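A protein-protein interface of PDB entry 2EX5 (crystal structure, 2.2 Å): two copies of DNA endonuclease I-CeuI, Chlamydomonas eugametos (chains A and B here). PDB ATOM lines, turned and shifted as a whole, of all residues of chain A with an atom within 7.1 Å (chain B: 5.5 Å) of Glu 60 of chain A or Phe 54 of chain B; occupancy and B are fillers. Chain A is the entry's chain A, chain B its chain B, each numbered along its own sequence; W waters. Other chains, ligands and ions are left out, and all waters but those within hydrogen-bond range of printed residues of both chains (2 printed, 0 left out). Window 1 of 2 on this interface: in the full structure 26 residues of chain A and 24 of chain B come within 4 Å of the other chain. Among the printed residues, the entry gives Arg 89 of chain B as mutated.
The backbone carbonyl oxygen (O) of Gly 57 of chain B lies close to the backbone NH (N) of Phe 58 of chain A (3.5 Å).
NH2 of Arg 89 of chain B lies within salt-bridge range of OE1 of Glu 60 of chain A.
OE2 of Glu 60 of chain A sits at hydrogen-bond distance from OG of Ser 145 of chain A (2.5 Å).
The backbone NH of Ser 146 of chain A is in hydrogen-bond range of the side-chain carboxylate of Glu 60 of chain A (3.3 Å).
The side-chain hydroxyl (OG) of Ser 146 of chain A sits at hydrogen-bond distance from the backbone NH (N) of Lys 149 of chain A, at 3.4 Å.
CG of Glu 50 of chain B touches CD2 of Leu 53 of chain A, 3.5 Å away.
Phe 54 of chain B touches Leu 53 of chain A.
Phe 54 of chain B touches Ala 56 of chain A (CE1 to O, 3.7 Å).
C of Gly 57 of chain B touches C of Gly 57 of chain A, 3.5 Å away.
C of Gly 57 of chain A touches N of Phe 58 of chain B (3.3 Å).
Phe 58 of chain A touches Phe 58 of chain B (N to N, 3.7 Å).
Glu 60 of chain A touches Val 96 of chain B (OE1 to CG2, 3.8 Å).
O of Val 141 of chain A touches CE1 of Phe 54 of chain B (3.8 Å).
Ser 51 of chain B touches Phe 144 of chain A.
Lys 149 of chain A touches Arg 89 of chain B.
Of chain B, only Phe 54, Arg 89 and Val 96 come within 4 Å of Glu 60 of chain A.
Printed residues of chain B within 4 Å of Ala 56 of chain A: Phe 54 (3.7 Å).
Of the printed residues of chain A, Phe 58 of chain B touches Gly 57 and Phe 58.
Of the printed residues of chain B, Phe 54 of chain A touches Leu 53, Ala 56 and Gly 57.
Printed residues of chain B within 4 Å of Gly 57 of chain A: Phe 54 (3.1 Å), Gly 57 (3.5 Å) and Phe 58 (3.3 Å).
Val 150 of chain A touches none of the printed residues of chain B.
The nearest residue of chain A that does not touch Phe 54 of chain B is Tyr 140 of chain A (4.3 Å).
The nearest printed residue of chain B that does not touch Ala 56 of chain A is Phe 58 of chain B (5.9 Å).
Of the 13 printed residues of chain B, 9 touch a printed residue of chain A.
Of the 24 printed residues of chain A, 10 touch a printed residue of chain B.
Printed residues of chain A that touch a printed residue of chain B: Glu 50, Leu 53, Phe 54, Ala 56, Gly 57, Phe 58, Glu 60, Val 141, Phe 144 and Lys 149.
Hydrophobic or aromatic side chains of chain A that line the printed part of chain B: Leu 53, Phe 54, Ala 56, Phe 58 and Phe 144.
Among the printed residues, 21 pairs touch across the chains.
Glu 50 of chain A touches Leu 53 of chain B, and with the chains exchanged Leu 53 of chain A touches Glu 50 of chain B.
Leu 53 of chain B touches its own counterpart, Leu 53 of chain A.
Leu 53 of chain A touches Phe 54 of chain B, and with the chains exchanged Phe 54 of chain A touches Leu 53 of chain B.
Phe 58 of chain A touches its own counterpart, Phe 58 of chain B.
Positions printed for both chains: 50, 52, 53, 54, 55, 56, 57, 58 and 59.
Of the 21 pairs that touch across the chains among the printed residues, 13 have their exchanged pair printed and touching as well.
Water W2 bridges O of Gly 61 of chain A (2.4 Å) and NH1 of Arg 89 of chain B (2.8 Å).
Water W1 lies within hydrogen-bond range of OE1 of Glu 60 of chain A (2.6 Å) and NE of Arg 89 of chain B (2.8 Å).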
ATOM      1  N   GLU A  50     -12.503 -16.383  16.194  1.00  0.00           N
ATOM      2  CA  GLU A  50     -13.095 -17.641  16.663  1.00  0.00           C
ATOM      3  C   GLU A  50     -14.506 -17.972  16.040  1.00  0.00           C
ATOM      4  O   GLU A  50     -14.757 -19.131  15.637  1.00  0.00           O
ATOM      5  CB  GLU A  50     -13.341 -17.491  18.103  1.00  0.00           C
ATOM      6  CG  GLU A  50     -12.748 -18.533  18.946  1.00  0.00           C
ATOM      7  CD  GLU A  50     -11.498 -18.027  19.626  1.00  0.00           C
ATOM      8  OE1 GLU A  50     -10.929 -16.962  19.185  1.00  0.00           O
ATOM      9  OE2 GLU A  50     -11.104 -18.676  20.618  1.00  0.00           O
ATOM     10  N   LYS A  52     -15.840 -16.671  13.328  1.00  0.00           N
ATOM     11  CA  LYS A  52     -15.557 -16.792  11.938  1.00  0.00           C
ATOM     12  C   LYS A  52     -15.065 -18.163  11.450  1.00  0.00           C
ATOM     13  O   LYS A  52     -15.453 -18.651  10.330  1.00  0.00           O
ATOM     14  CB  LYS A  52     -14.543 -15.752  11.581  1.00  0.00           C
ATOM     15  CG  LYS A  52     -15.148 -14.357  11.656  1.00  0.00           C
ATOM     16  CD  LYS A  52     -14.545 -13.452  10.632  1.00  0.00           C
ATOM     17  CE  LYS A  52     -13.977 -12.191  11.220  1.00  0.00           C
ATOM     18  NZ  LYS A  52     -13.037 -12.715  12.181  1.00  0.00           N
ATOM     19  N   LEU A  53     -14.202 -18.777  12.259  1.00  0.00           N
ATOM     20  CA  LEU A  53     -13.717 -20.109  11.960  1.00  0.00           C
ATOM     21  C   LEU A  53     -14.859 -21.094  12.111  1.00  0.00           C
ATOM     22  O   LEU A  53     -14.870 -22.051  11.430  1.00  0.00           O
ATOM     23  CB  LEU A  53     -12.519 -20.527  12.874  1.00  0.00           C
ATOM     24  CG  LEU A  53     -11.006 -20.453  12.579  1.00  0.00           C
ATOM     25  CD1 LEU A  53     -10.606 -19.880  11.294  1.00  0.00           C
ATOM     26  CD2 LEU A  53     -10.086 -19.819  13.742  1.00  0.00           C
ATOM     27  N   PHE A  54     -15.718 -20.900  13.112  1.00  0.00           N
ATOM     28  CA  PHE A  54     -16.913 -21.708  13.366  1.00  0.00           C
ATOM     29  C   PHE A  54     -17.891 -21.494  12.156  1.00  0.00           C
ATOM     30  O   PHE A  54     -18.415 -22.444  11.628  1.00  0.00           O
ATOM     31  CB  PHE A  54     -17.591 -21.327  14.705  1.00  0.00           C
ATOM     32  CG  PHE A  54     -18.935 -22.094  14.996  1.00  0.00           C
ATOM     33  CD1 PHE A  54     -18.936 -23.271  15.739  1.00  0.00           C
ATOM     34  CD2 PHE A  54     -20.142 -21.644  14.481  1.00  0.00           C
ATOM     35  CE1 PHE A  54     -20.133 -23.982  16.021  1.00  0.00           C
ATOM     36  CE2 PHE A  54     -21.295 -22.340  14.718  1.00  0.00           C
ATOM     37  CZ  PHE A  54     -21.293 -23.490  15.489  1.00  0.00           C
ATOM     38  N   LEU A  55     -18.061 -20.269  11.665  1.00  0.00           N
ATOM     39  CA  LEU A  55     -18.924 -20.088  10.571  1.00  0.00           C
ATOM     40  C   LEU A  55     -18.310 -20.773   9.329  1.00  0.00           C
ATOM     41  O   LEU A  55     -19.056 -21.309   8.542  1.00  0.00           O
ATOM     42  CB  LEU A  55     -19.160 -18.629  10.334  1.00  0.00           C
ATOM     43  CG  LEU A  55     -19.915 -18.095   9.098  1.00  0.00           C
ATOM     44  CD1 LEU A  55     -21.416 -18.625   9.174  1.00  0.00           C
ATOM     45  CD2 LEU A  55     -19.841 -16.577   8.993  1.00  0.00           C
ATOM     46  N   ALA A  56     -16.975 -20.752   9.150  1.00  0.00           N
ATOM     47  CA  ALA A  56     -16.320 -21.420   8.024  1.00  0.00           C
ATOM     48  C   ALA A  56     -16.729 -22.880   7.976  1.00  0.00           C
ATOM     49  O   ALA A  56     -17.161 -23.338   6.933  1.00  0.00           O
ATOM     50  CB  ALA A  56     -14.807 -21.273   8.024  1.00  0.00           C
ATOM     51  N   GLY A  57     -16.713 -23.578   9.086  1.00  0.00           N
ATOM     52  CA  GLY A  57     -17.079 -25.007   9.136  1.00  0.00           C
ATOM     53  C   GLY A  57     -18.544 -25.160   8.831  1.00  0.00           C
ATOM     54  O   GLY A  57     -19.005 -26.081   8.124  1.00  0.00           O
ATOM     55  N   PHE A  58     -19.334 -24.225   9.313  1.00  0.00           N
ATOM     56  CA  PHE A  58     -20.780 -24.330   9.088  1.00  0.00           C
ATOM     57  C   PHE A  58     -21.126 -24.234   7.568  1.00  0.00           C
ATOM     58  O   PHE A  58     -22.020 -24.891   7.101  1.00  0.00           O
ATOM     59  CB  PHE A  58     -21.400 -23.166   9.817  1.00  0.00           C
ATOM     60  CG  PHE A  58     -22.852 -23.131   9.730  1.00  0.00           C
ATOM     61  CD1 PHE A  58     -23.602 -24.007  10.466  1.00  0.00           C
ATOM     62  CD2 PHE A  58     -23.494 -22.207   8.929  1.00  0.00           C
ATOM     63  CE1 PHE A  58     -24.936 -23.939  10.420  1.00  0.00           C
ATOM     64  CE2 PHE A  58     -24.848 -22.196   8.842  1.00  0.00           C
ATOM     65  CZ  PHE A  58     -25.540 -23.068   9.581  1.00  0.00           C
ATOM     66  N   LEU A  59     -20.449 -23.314   6.871  1.00  0.00           N
ATOM     67  CA  LEU A  59     -20.682 -23.023   5.504  1.00  0.00           C
ATOM     68  C   LEU A  59     -20.189 -24.150   4.588  1.00  0.00           C
ATOM     69  O   LEU A  59     -20.801 -24.382   3.506  1.00  0.00           O
ATOM     70  CB  LEU A  59     -19.930 -21.740   5.123  1.00  0.00           C
ATOM     71  CG  LEU A  59     -20.313 -20.343   5.646  1.00  0.00           C
ATOM     72  CD1 LEU A  59     -19.501 -19.319   4.768  1.00  0.00           C
ATOM     73  CD2 LEU A  59     -21.816 -20.160   5.558  1.00  0.00           C
ATOM     74  N   GLU A  60     -19.079 -24.788   4.975  1.00  0.00           N
ATOM     75  CA  GLU A  60     -18.627 -26.018   4.325  1.00  0.00           C
ATOM     76  C   GLU A  60     -19.754 -27.053   4.340  1.00  0.00           C
ATOM     77  O   GLU A  60     -19.930 -27.750   3.398  1.00  0.00           O
ATOM     78  CB  GLU A  60     -17.341 -26.559   4.952  1.00  0.00           C
ATOM     79  CG  GLU A  60     -16.850 -27.896   4.517  1.00  0.00           C
ATOM     80  CD  GLU A  60     -16.033 -27.834   3.260  1.00  0.00           C
ATOM     81  OE1 GLU A  60     -15.605 -28.960   2.825  1.00  0.00           O
ATOM     82  OE2 GLU A  60     -15.867 -26.685   2.701  1.00  0.00           O
ATOM     83  N   GLY A  61     -20.516 -27.054   5.440  1.00  0.00           N
ATOM     84  CA  GLY A  61     -21.675 -27.865   5.659  1.00  0.00           C
ATOM     85  C   GLY A  61     -22.952 -27.470   4.949  1.00  0.00           C
ATOM     86  O   GLY A  61     -23.588 -28.358   4.430  1.00  0.00           O
ATOM     87  N   GLU A  62     -23.356 -26.190   4.959  1.00  0.00           N
ATOM     88  CA  GLU A  62     -24.747 -25.814   4.743  1.00  0.00           C
ATOM     89  C   GLU A  62     -24.927 -24.758   3.614  1.00  0.00           C
ATOM     90  O   GLU A  62     -26.049 -24.358   3.293  1.00  0.00           O
ATOM     91  CB  GLU A  62     -25.316 -25.220   6.045  1.00  0.00           C
ATOM     92  CG  GLU A  62     -25.199 -26.050   7.333  1.00  0.00           C
ATOM     93  CD  GLU A  62     -26.281 -27.054   7.463  1.00  0.00           C
ATOM     94  OE1 GLU A  62     -26.522 -27.719   6.462  1.00  0.00           O
ATOM     95  OE2 GLU A  62     -26.938 -27.181   8.528  1.00  0.00           O
ATOM     96  N   ALA A  63     -23.810 -24.222   3.125  1.00  0.00           N
ATOM     97  CA  ALA A  63     -23.794 -23.094   2.170  1.00  0.00           C
ATOM     98  C   ALA A  63     -23.565 -23.667   0.770  1.00  0.00           C
ATOM     99  O   ALA A  63     -23.141 -24.809   0.603  1.00  0.00           O
ATOM    100  CB  ALA A  63     -22.644 -22.160   2.530  1.00  0.00           C
ATOM    101  N   TYR A 137     -14.205 -16.894   2.091  1.00  0.00           N
ATOM    102  CA  TYR A 137     -13.944 -18.303   1.797  1.00  0.00           C
ATOM    103  C   TYR A 137     -12.450 -18.504   1.733  1.00  0.00           C
ATOM    104  O   TYR A 137     -11.945 -19.542   2.174  1.00  0.00           O
ATOM    105  CB  TYR A 137     -14.631 -18.736   0.457  1.00  0.00           C
ATOM    106  CG  TYR A 137     -16.001 -19.400   0.647  1.00  0.00           C
ATOM    107  CD1 TYR A 137     -16.126 -20.795   0.867  1.00  0.00           C
ATOM    108  CD2 TYR A 137     -17.170 -18.622   0.652  1.00  0.00           C
ATOM    109  CE1 TYR A 137     -17.438 -21.408   1.066  1.00  0.00           C
ATOM    110  CE2 TYR A 137     -18.454 -19.193   0.827  1.00  0.00           C
ATOM    111  CZ  TYR A 137     -18.595 -20.565   1.011  1.00  0.00           C
ATOM    112  OH  TYR A 137     -19.892 -21.046   1.142  1.00  0.00           O
ATOM    113  N   TYR A 140     -10.913 -17.866   5.569  1.00  0.00           N
ATOM    114  CA  TYR A 140     -11.299 -18.881   6.584  1.00  0.00           C
ATOM    115  C   TYR A 140     -11.696 -20.247   6.162  1.00  0.00           C
ATOM    116  O   TYR A 140     -11.631 -21.112   6.968  1.00  0.00           O
ATOM    117  CB  TYR A 140     -12.404 -18.387   7.536  1.00  0.00           C
ATOM    118  CG  TYR A 140     -12.053 -17.120   8.197  1.00  0.00           C
ATOM    119  CD1 TYR A 140     -12.378 -15.874   7.604  1.00  0.00           C
ATOM    120  CD2 TYR A 140     -11.309 -17.149   9.418  1.00  0.00           C
ATOM    121  CE1 TYR A 140     -11.973 -14.667   8.252  1.00  0.00           C
ATOM    122  CE2 TYR A 140     -10.900 -15.994  10.029  1.00  0.00           C
ATOM    123  CZ  TYR A 140     -11.234 -14.781   9.462  1.00  0.00           C
ATOM    124  OH  TYR A 140     -10.847 -13.710  10.161  1.00  0.00           O
ATOM    125  N   VAL A 141     -12.289 -20.416   4.981  1.00  0.00           N
ATOM    126  CA  VAL A 141     -12.798 -21.761   4.563  1.00  0.00           C
ATOM    127  C   VAL A 141     -11.775 -22.654   3.942  1.00  0.00           C
ATOM    128  O   VAL A 141     -11.633 -23.771   4.345  1.00  0.00           O
ATOM    129  CB  VAL A 141     -14.136 -21.700   3.617  1.00  0.00           C
ATOM    130  CG1 VAL A 141     -14.731 -23.121   3.372  1.00  0.00           C
ATOM    131  CG2 VAL A 141     -15.232 -20.856   4.300  1.00  0.00           C
ATOM    132  N   VAL A 142     -11.103 -22.186   2.890  1.00  0.00           N
ATOM    133  CA  VAL A 142     -10.509 -23.088   1.926  1.00  0.00           C
ATOM    134  C   VAL A 142      -9.381 -24.001   2.475  1.00  0.00           C
ATOM    135  O   VAL A 142      -9.142 -25.106   1.923  1.00  0.00           O
ATOM    136  CB  VAL A 142      -9.914 -22.299   0.741  1.00  0.00           C
ATOM    137  CG1 VAL A 142      -8.866 -23.231   0.055  1.00  0.00           C
ATOM    138  CG2 VAL A 142     -11.001 -21.813  -0.277  1.00  0.00           C
ATOM    139  N   ALA A 143      -8.723 -23.567   3.555  1.00  0.00           N
ATOM    140  CA  ALA A 143      -7.630 -24.310   4.194  1.00  0.00           C
ATOM    141  C   ALA A 143      -8.118 -25.639   4.738  1.00  0.00           C
ATOM    142  O   ALA A 143      -7.436 -26.678   4.676  1.00  0.00           O
ATOM    143  CB  ALA A 143      -6.984 -23.437   5.336  1.00  0.00           C
ATOM    144  N   PHE A 144      -9.331 -25.641   5.246  1.00  0.00           N
ATOM    145  CA  PHE A 144      -9.891 -26.876   5.794  1.00  0.00           C
ATOM    146  C   PHE A 144     -10.894 -27.524   4.844  1.00  0.00           C
ATOM    147  O   PHE A 144     -11.521 -28.518   5.167  1.00  0.00           O
ATOM    148  CB  PHE A 144     -10.551 -26.564   7.154  1.00  0.00           C
ATOM    149  CG  PHE A 144      -9.809 -25.535   7.993  1.00  0.00           C
ATOM    150  CD1 PHE A 144      -8.730 -25.898   8.810  1.00  0.00           C
ATOM    151  CD2 PHE A 144     -10.164 -24.209   7.958  1.00  0.00           C
ATOM    152  CE1 PHE A 144      -8.060 -24.950   9.642  1.00  0.00           C
ATOM    153  CE2 PHE A 144      -9.483 -23.247   8.769  1.00  0.00           C
ATOM    154  CZ  PHE A 144      -8.465 -23.651   9.624  1.00  0.00           C
ATOM    155  N   SER A 145     -11.074 -26.975   3.666  1.00  0.00           N
ATOM    156  CA  SER A 145     -12.086 -27.444   2.794  1.00  0.00           C
ATOM    157  C   SER A 145     -11.666 -28.661   1.942  1.00  0.00           C
ATOM    158  O   SER A 145     -10.485 -28.932   1.739  1.00  0.00           O
ATOM    159  CB  SER A 145     -12.500 -26.275   1.883  1.00  0.00           C
ATOM    160  OG  SER A 145     -13.791 -26.466   1.375  1.00  0.00           O
ATOM    161  N   SER A 146     -12.665 -29.391   1.456  1.00  0.00           N
ATOM    162  CA  SER A 146     -12.454 -30.552   0.539  1.00  0.00           C
ATOM    163  C   SER A 146     -11.979 -30.050  -0.795  1.00  0.00           C
ATOM    164  O   SER A 146     -12.265 -28.920  -1.164  1.00  0.00           O
ATOM    165  CB  SER A 146     -13.756 -31.400   0.357  1.00  0.00           C
ATOM    166  OG  SER A 146     -14.668 -30.687  -0.483  1.00  0.00           O
ATOM    167  N   PRO A 147     -11.172 -30.858  -1.515  1.00  0.00           N
ATOM    168  CA  PRO A 147     -10.846 -30.480  -2.872  1.00  0.00           C
ATOM    169  C   PRO A 147     -11.964 -29.957  -3.765  1.00  0.00           C
ATOM    170  O   PRO A 147     -11.747 -28.978  -4.453  1.00  0.00           O
ATOM    171  CB  PRO A 147     -10.189 -31.777  -3.445  1.00  0.00           C
ATOM    172  CG  PRO A 147      -9.368 -32.282  -2.203  1.00  0.00           C
ATOM    173  CD  PRO A 147     -10.404 -32.050  -1.073  1.00  0.00           C
ATOM    174  N   LYS A 149     -14.703 -28.433  -2.995  1.00  0.00           N
ATOM    175  CA  LYS A 149     -15.385 -27.175  -2.585  1.00  0.00           C
ATOM    176  C   LYS A 149     -14.421 -26.053  -2.889  1.00  0.00           C
ATOM    177  O   LYS A 149     -14.847 -25.053  -3.368  1.00  0.00           O
ATOM    178  CB  LYS A 149     -15.830 -27.166  -1.073  1.00  0.00           C
ATOM    179  CG  LYS A 149     -17.327 -27.370  -0.707  1.00  0.00           C
ATOM    180  CD  LYS A 149     -17.999 -28.497  -1.369  1.00  0.00           C
ATOM    181  CE  LYS A 149     -19.511 -28.234  -1.547  1.00  0.00           C
ATOM    182  NZ  LYS A 149     -20.290 -28.444  -0.314  1.00  0.00           N
ATOM    183  N   VAL A 150     -13.119 -26.273  -2.645  1.00  0.00           N
ATOM    184  CA  VAL A 150     -12.001 -25.362  -3.013  1.00  0.00           C
ATOM    185  C   VAL A 150     -12.047 -25.036  -4.470  1.00  0.00           C
ATOM    186  O   VAL A 150     -11.970 -23.874  -4.856  1.00  0.00           O
ATOM    187  CB  VAL A 150     -10.546 -25.958  -2.644  1.00  0.00           C
ATOM    188  CG1 VAL A 150      -9.375 -25.081  -3.112  1.00  0.00           C
ATOM    189  CG2 VAL A 150     -10.460 -26.249  -1.225  1.00  0.00           C
ATOM    190  N   GLU B  50      -7.647 -23.788  15.468  1.00  0.00           N
ATOM    191  CA  GLU B  50      -8.397 -23.266  14.386  1.00  0.00           C
ATOM    192  C   GLU B  50      -9.214 -24.337  13.605  1.00  0.00           C
ATOM    193  O   GLU B  50     -10.376 -24.117  13.300  1.00  0.00           O
ATOM    194  CB  GLU B  50      -7.441 -22.552  13.431  1.00  0.00           C
ATOM    195  CG  GLU B  50      -6.870 -21.259  14.020  1.00  0.00           C
ATOM    196  CD  GLU B  50      -5.421 -21.454  14.343  1.00  0.00           C
ATOM    197  OE1 GLU B  50      -5.052 -21.404  15.528  1.00  0.00           O
ATOM    198  OE2 GLU B  50      -4.652 -21.759  13.382  1.00  0.00           O
ATOM    199  N   SER B  51      -8.550 -25.450  13.267  1.00  0.00           N
ATOM    200  CA  SER B  51      -9.144 -26.590  12.570  1.00  0.00           C
ATOM    201  C   SER B  51     -10.236 -27.160  13.440  1.00  0.00           C
ATOM    202  O   SER B  51     -11.207 -27.663  12.953  1.00  0.00           O
ATOM    203  CB  SER B  51      -8.080 -27.641  12.235  1.00  0.00           C
ATOM    204  OG  SER B  51      -7.844 -28.513  13.337  1.00  0.00           O
ATOM    205  N   LYS B  52     -10.109 -26.997  14.755  1.00  0.00           N
ATOM    206  CA  LYS B  52     -11.117 -27.472  15.669  1.00  0.00           C
ATOM    207  C   LYS B  52     -12.370 -26.598  15.740  1.00  0.00           C
ATOM    208  O   LYS B  52     -13.461 -27.106  15.902  1.00  0.00           O
ATOM    209  CB  LYS B  52     -10.557 -27.617  17.069  1.00  0.00           C
ATOM    210  CG  LYS B  52      -9.757 -28.864  17.370  1.00  0.00           C
ATOM    211  CD  LYS B  52      -8.716 -28.398  18.402  1.00  0.00           C
ATOM    212  CE  LYS B  52      -8.048 -29.425  19.255  1.00  0.00           C
ATOM    213  NZ  LYS B  52      -6.911 -28.623  19.994  1.00  0.00           N
ATOM    214  N   LEU B  53     -12.217 -25.304  15.725  1.00  0.00           N
ATOM    215  CA  LEU B  53     -13.352 -24.395  15.495  1.00  0.00           C
ATOM    216  C   LEU B  53     -14.066 -24.656  14.110  1.00  0.00           C
ATOM    217  O   LEU B  53     -15.211 -24.767  14.067  1.00  0.00           O
ATOM    218  CB  LEU B  53     -12.808 -22.967  15.512  1.00  0.00           C
ATOM    219  CG  LEU B  53     -12.554 -22.112  16.765  1.00  0.00           C
ATOM    220  CD1 LEU B  53     -13.407 -22.463  17.971  1.00  0.00           C
ATOM    221  CD2 LEU B  53     -11.062 -21.999  16.994  1.00  0.00           C
ATOM    222  N   PHE B  54     -13.336 -24.828  13.039  1.00  0.00           N
ATOM    223  CA  PHE B  54     -13.842 -25.299  11.794  1.00  0.00           C
ATOM    224  C   PHE B  54     -14.659 -26.582  11.892  1.00  0.00           C
ATOM    225  O   PHE B  54     -15.830 -26.653  11.448  1.00  0.00           O
ATOM    226  CB  PHE B  54     -12.717 -25.401  10.725  1.00  0.00           C
ATOM    227  CG  PHE B  54     -13.251 -25.767   9.282  1.00  0.00           C
ATOM    228  CD1 PHE B  54     -13.451 -24.784   8.322  1.00  0.00           C
ATOM    229  CD2 PHE B  54     -13.634 -27.107   8.951  1.00  0.00           C
ATOM    230  CE1 PHE B  54     -13.946 -25.120   6.978  1.00  0.00           C
ATOM    231  CE2 PHE B  54     -14.150 -27.428   7.672  1.00  0.00           C
ATOM    232  CZ  PHE B  54     -14.259 -26.446   6.674  1.00  0.00           C
ATOM    233  N   LEU B  55     -14.102 -27.587  12.530  1.00  0.00           N
ATOM    234  CA  LEU B  55     -14.853 -28.746  12.847  1.00  0.00           C
ATOM    235  C   LEU B  55     -16.112 -28.490  13.620  1.00  0.00           C
ATOM    236  O   LEU B  55     -17.136 -29.024  13.296  1.00  0.00           O
ATOM    237  CB  LEU B  55     -13.981 -29.720  13.579  1.00  0.00           C
ATOM    238  CG  LEU B  55     -14.470 -31.171  13.728  1.00  0.00           C
ATOM    239  CD1 LEU B  55     -14.481 -31.803  12.310  1.00  0.00           C
ATOM    240  CD2 LEU B  55     -13.510 -31.915  14.742  1.00  0.00           C
ATOM    241  N   ALA B  56     -16.004 -27.735  14.711  1.00  0.00           N
ATOM    242  CA  ALA B  56     -17.134 -27.416  15.544  1.00  0.00           C
ATOM    243  C   ALA B  56     -18.327 -26.855  14.744  1.00  0.00           C
ATOM    244  O   ALA B  56     -19.485 -27.339  14.980  1.00  0.00           O
ATOM    245  CB  ALA B  56     -16.693 -26.395  16.700  1.00  0.00           C
ATOM    246  N   GLY B  57     -18.056 -25.897  13.817  1.00  0.00           N
ATOM    247  CA  GLY B  57     -19.164 -25.302  12.988  1.00  0.00           C
ATOM    248  C   GLY B  57     -19.691 -26.337  11.971  1.00  0.00           C
ATOM    249  O   GLY B  57     -20.837 -26.352  11.601  1.00  0.00           O
ATOM    250  N   PHE B  58     -18.791 -27.191  11.460  1.00  0.00           N
ATOM    251  CA  PHE B  58     -19.188 -28.317  10.642  1.00  0.00           C
ATOM    252  C   PHE B  58     -20.109 -29.280  11.364  1.00  0.00           C
ATOM    253  O   PHE B  58     -21.042 -29.784  10.759  1.00  0.00           O
ATOM    254  CB  PHE B  58     -17.961 -29.035  10.127  1.00  0.00           C
ATOM    255  CG  PHE B  58     -18.273 -30.137   9.183  1.00  0.00           C
ATOM    256  CD1 PHE B  58     -18.619 -29.836   7.845  1.00  0.00           C
ATOM    257  CD2 PHE B  58     -18.263 -31.485   9.656  1.00  0.00           C
ATOM    258  CE1 PHE B  58     -18.990 -30.901   6.955  1.00  0.00           C
ATOM    259  CE2 PHE B  58     -18.603 -32.582   8.771  1.00  0.00           C
ATOM    260  CZ  PHE B  58     -18.989 -32.284   7.437  1.00  0.00           C
ATOM    261  N   LEU B  59     -19.878 -29.587  12.646  1.00  0.00           N
ATOM    262  CA  LEU B  59     -20.737 -30.465  13.369  1.00  0.00           C
ATOM    263  C   LEU B  59     -22.087 -29.824  13.624  1.00  0.00           C
ATOM    264  O   LEU B  59     -23.113 -30.508  13.704  1.00  0.00           O
ATOM    265  CB  LEU B  59     -20.095 -30.819  14.726  1.00  0.00           C
ATOM    266  CG  LEU B  59     -18.677 -31.433  14.781  1.00  0.00           C
ATOM    267  CD1 LEU B  59     -18.251 -31.816  16.271  1.00  0.00           C
ATOM    268  CD2 LEU B  59     -18.545 -32.598  13.754  1.00  0.00           C
ATOM    269  N   ARG B  89     -21.346 -37.616   5.192  1.00  0.00           N
ATOM    270  CA  ARG B  89     -20.786 -36.742   4.201  1.00  0.00           C
ATOM    271  C   ARG B  89     -20.524 -37.625   2.976  1.00  0.00           C
ATOM    272  O   ARG B  89     -20.118 -38.721   3.141  1.00  0.00           O
ATOM    273  CB  ARG B  89     -19.468 -36.137   4.704  1.00  0.00           C
ATOM    274  CG  ARG B  89     -18.875 -35.092   3.811  1.00  0.00           C
ATOM    275  CD  ARG B  89     -19.404 -33.746   4.278  1.00  0.00           C
ATOM    276  NE  ARG B  89     -18.910 -32.619   3.496  1.00  0.00           N
ATOM    277  CZ  ARG B  89     -19.667 -31.543   3.213  1.00  0.00           C
ATOM    278  NH1 ARG B  89     -20.966 -31.456   3.666  1.00  0.00           N
ATOM    279  NH2 ARG B  89     -19.150 -30.558   2.469  1.00  0.00           N
ATOM    280  N   VAL B  96     -13.009 -33.823   5.805  1.00  0.00           N
ATOM    281  CA  VAL B  96     -13.525 -33.178   7.028  1.00  0.00           C
ATOM    282  C   VAL B  96     -13.919 -34.242   8.061  1.00  0.00           C
ATOM    283  O   VAL B  96     -13.844 -34.021   9.299  1.00  0.00           O
ATOM    284  CB  VAL B  96     -14.685 -32.205   6.677  1.00  0.00           C
ATOM    285  CG1 VAL B  96     -15.166 -31.435   7.904  1.00  0.00           C
ATOM    286  CG2 VAL B  96     -14.233 -31.185   5.589  1.00  0.00           C
ATOM    287  N   LEU B  99     -10.646 -35.258   9.532  1.00  0.00           N
ATOM    288  CA  LEU B  99     -10.330 -34.272  10.560  1.00  0.00           C
ATOM    289  C   LEU B  99     -10.982 -34.668  11.868  1.00  0.00           C
ATOM    290  O   LEU B  99     -10.340 -34.713  12.906  1.00  0.00           O
ATOM    291  CB  LEU B  99     -10.833 -32.864  10.096  1.00  0.00           C
ATOM    292  CG  LEU B  99     -10.268 -31.520  10.536  1.00  0.00           C
ATOM    293  CD1 LEU B  99     -11.392 -30.522  10.805  1.00  0.00           C
ATOM    294  CD2 LEU B  99      -9.211 -31.541  11.718  1.00  0.00           C
HETATM  295  O   HOH W   1     -16.477 -31.369   3.052  1.00  0.00           O
HETATM  296  O   HOH W   2     -23.493 -30.361   3.051  1.00  0.00           O
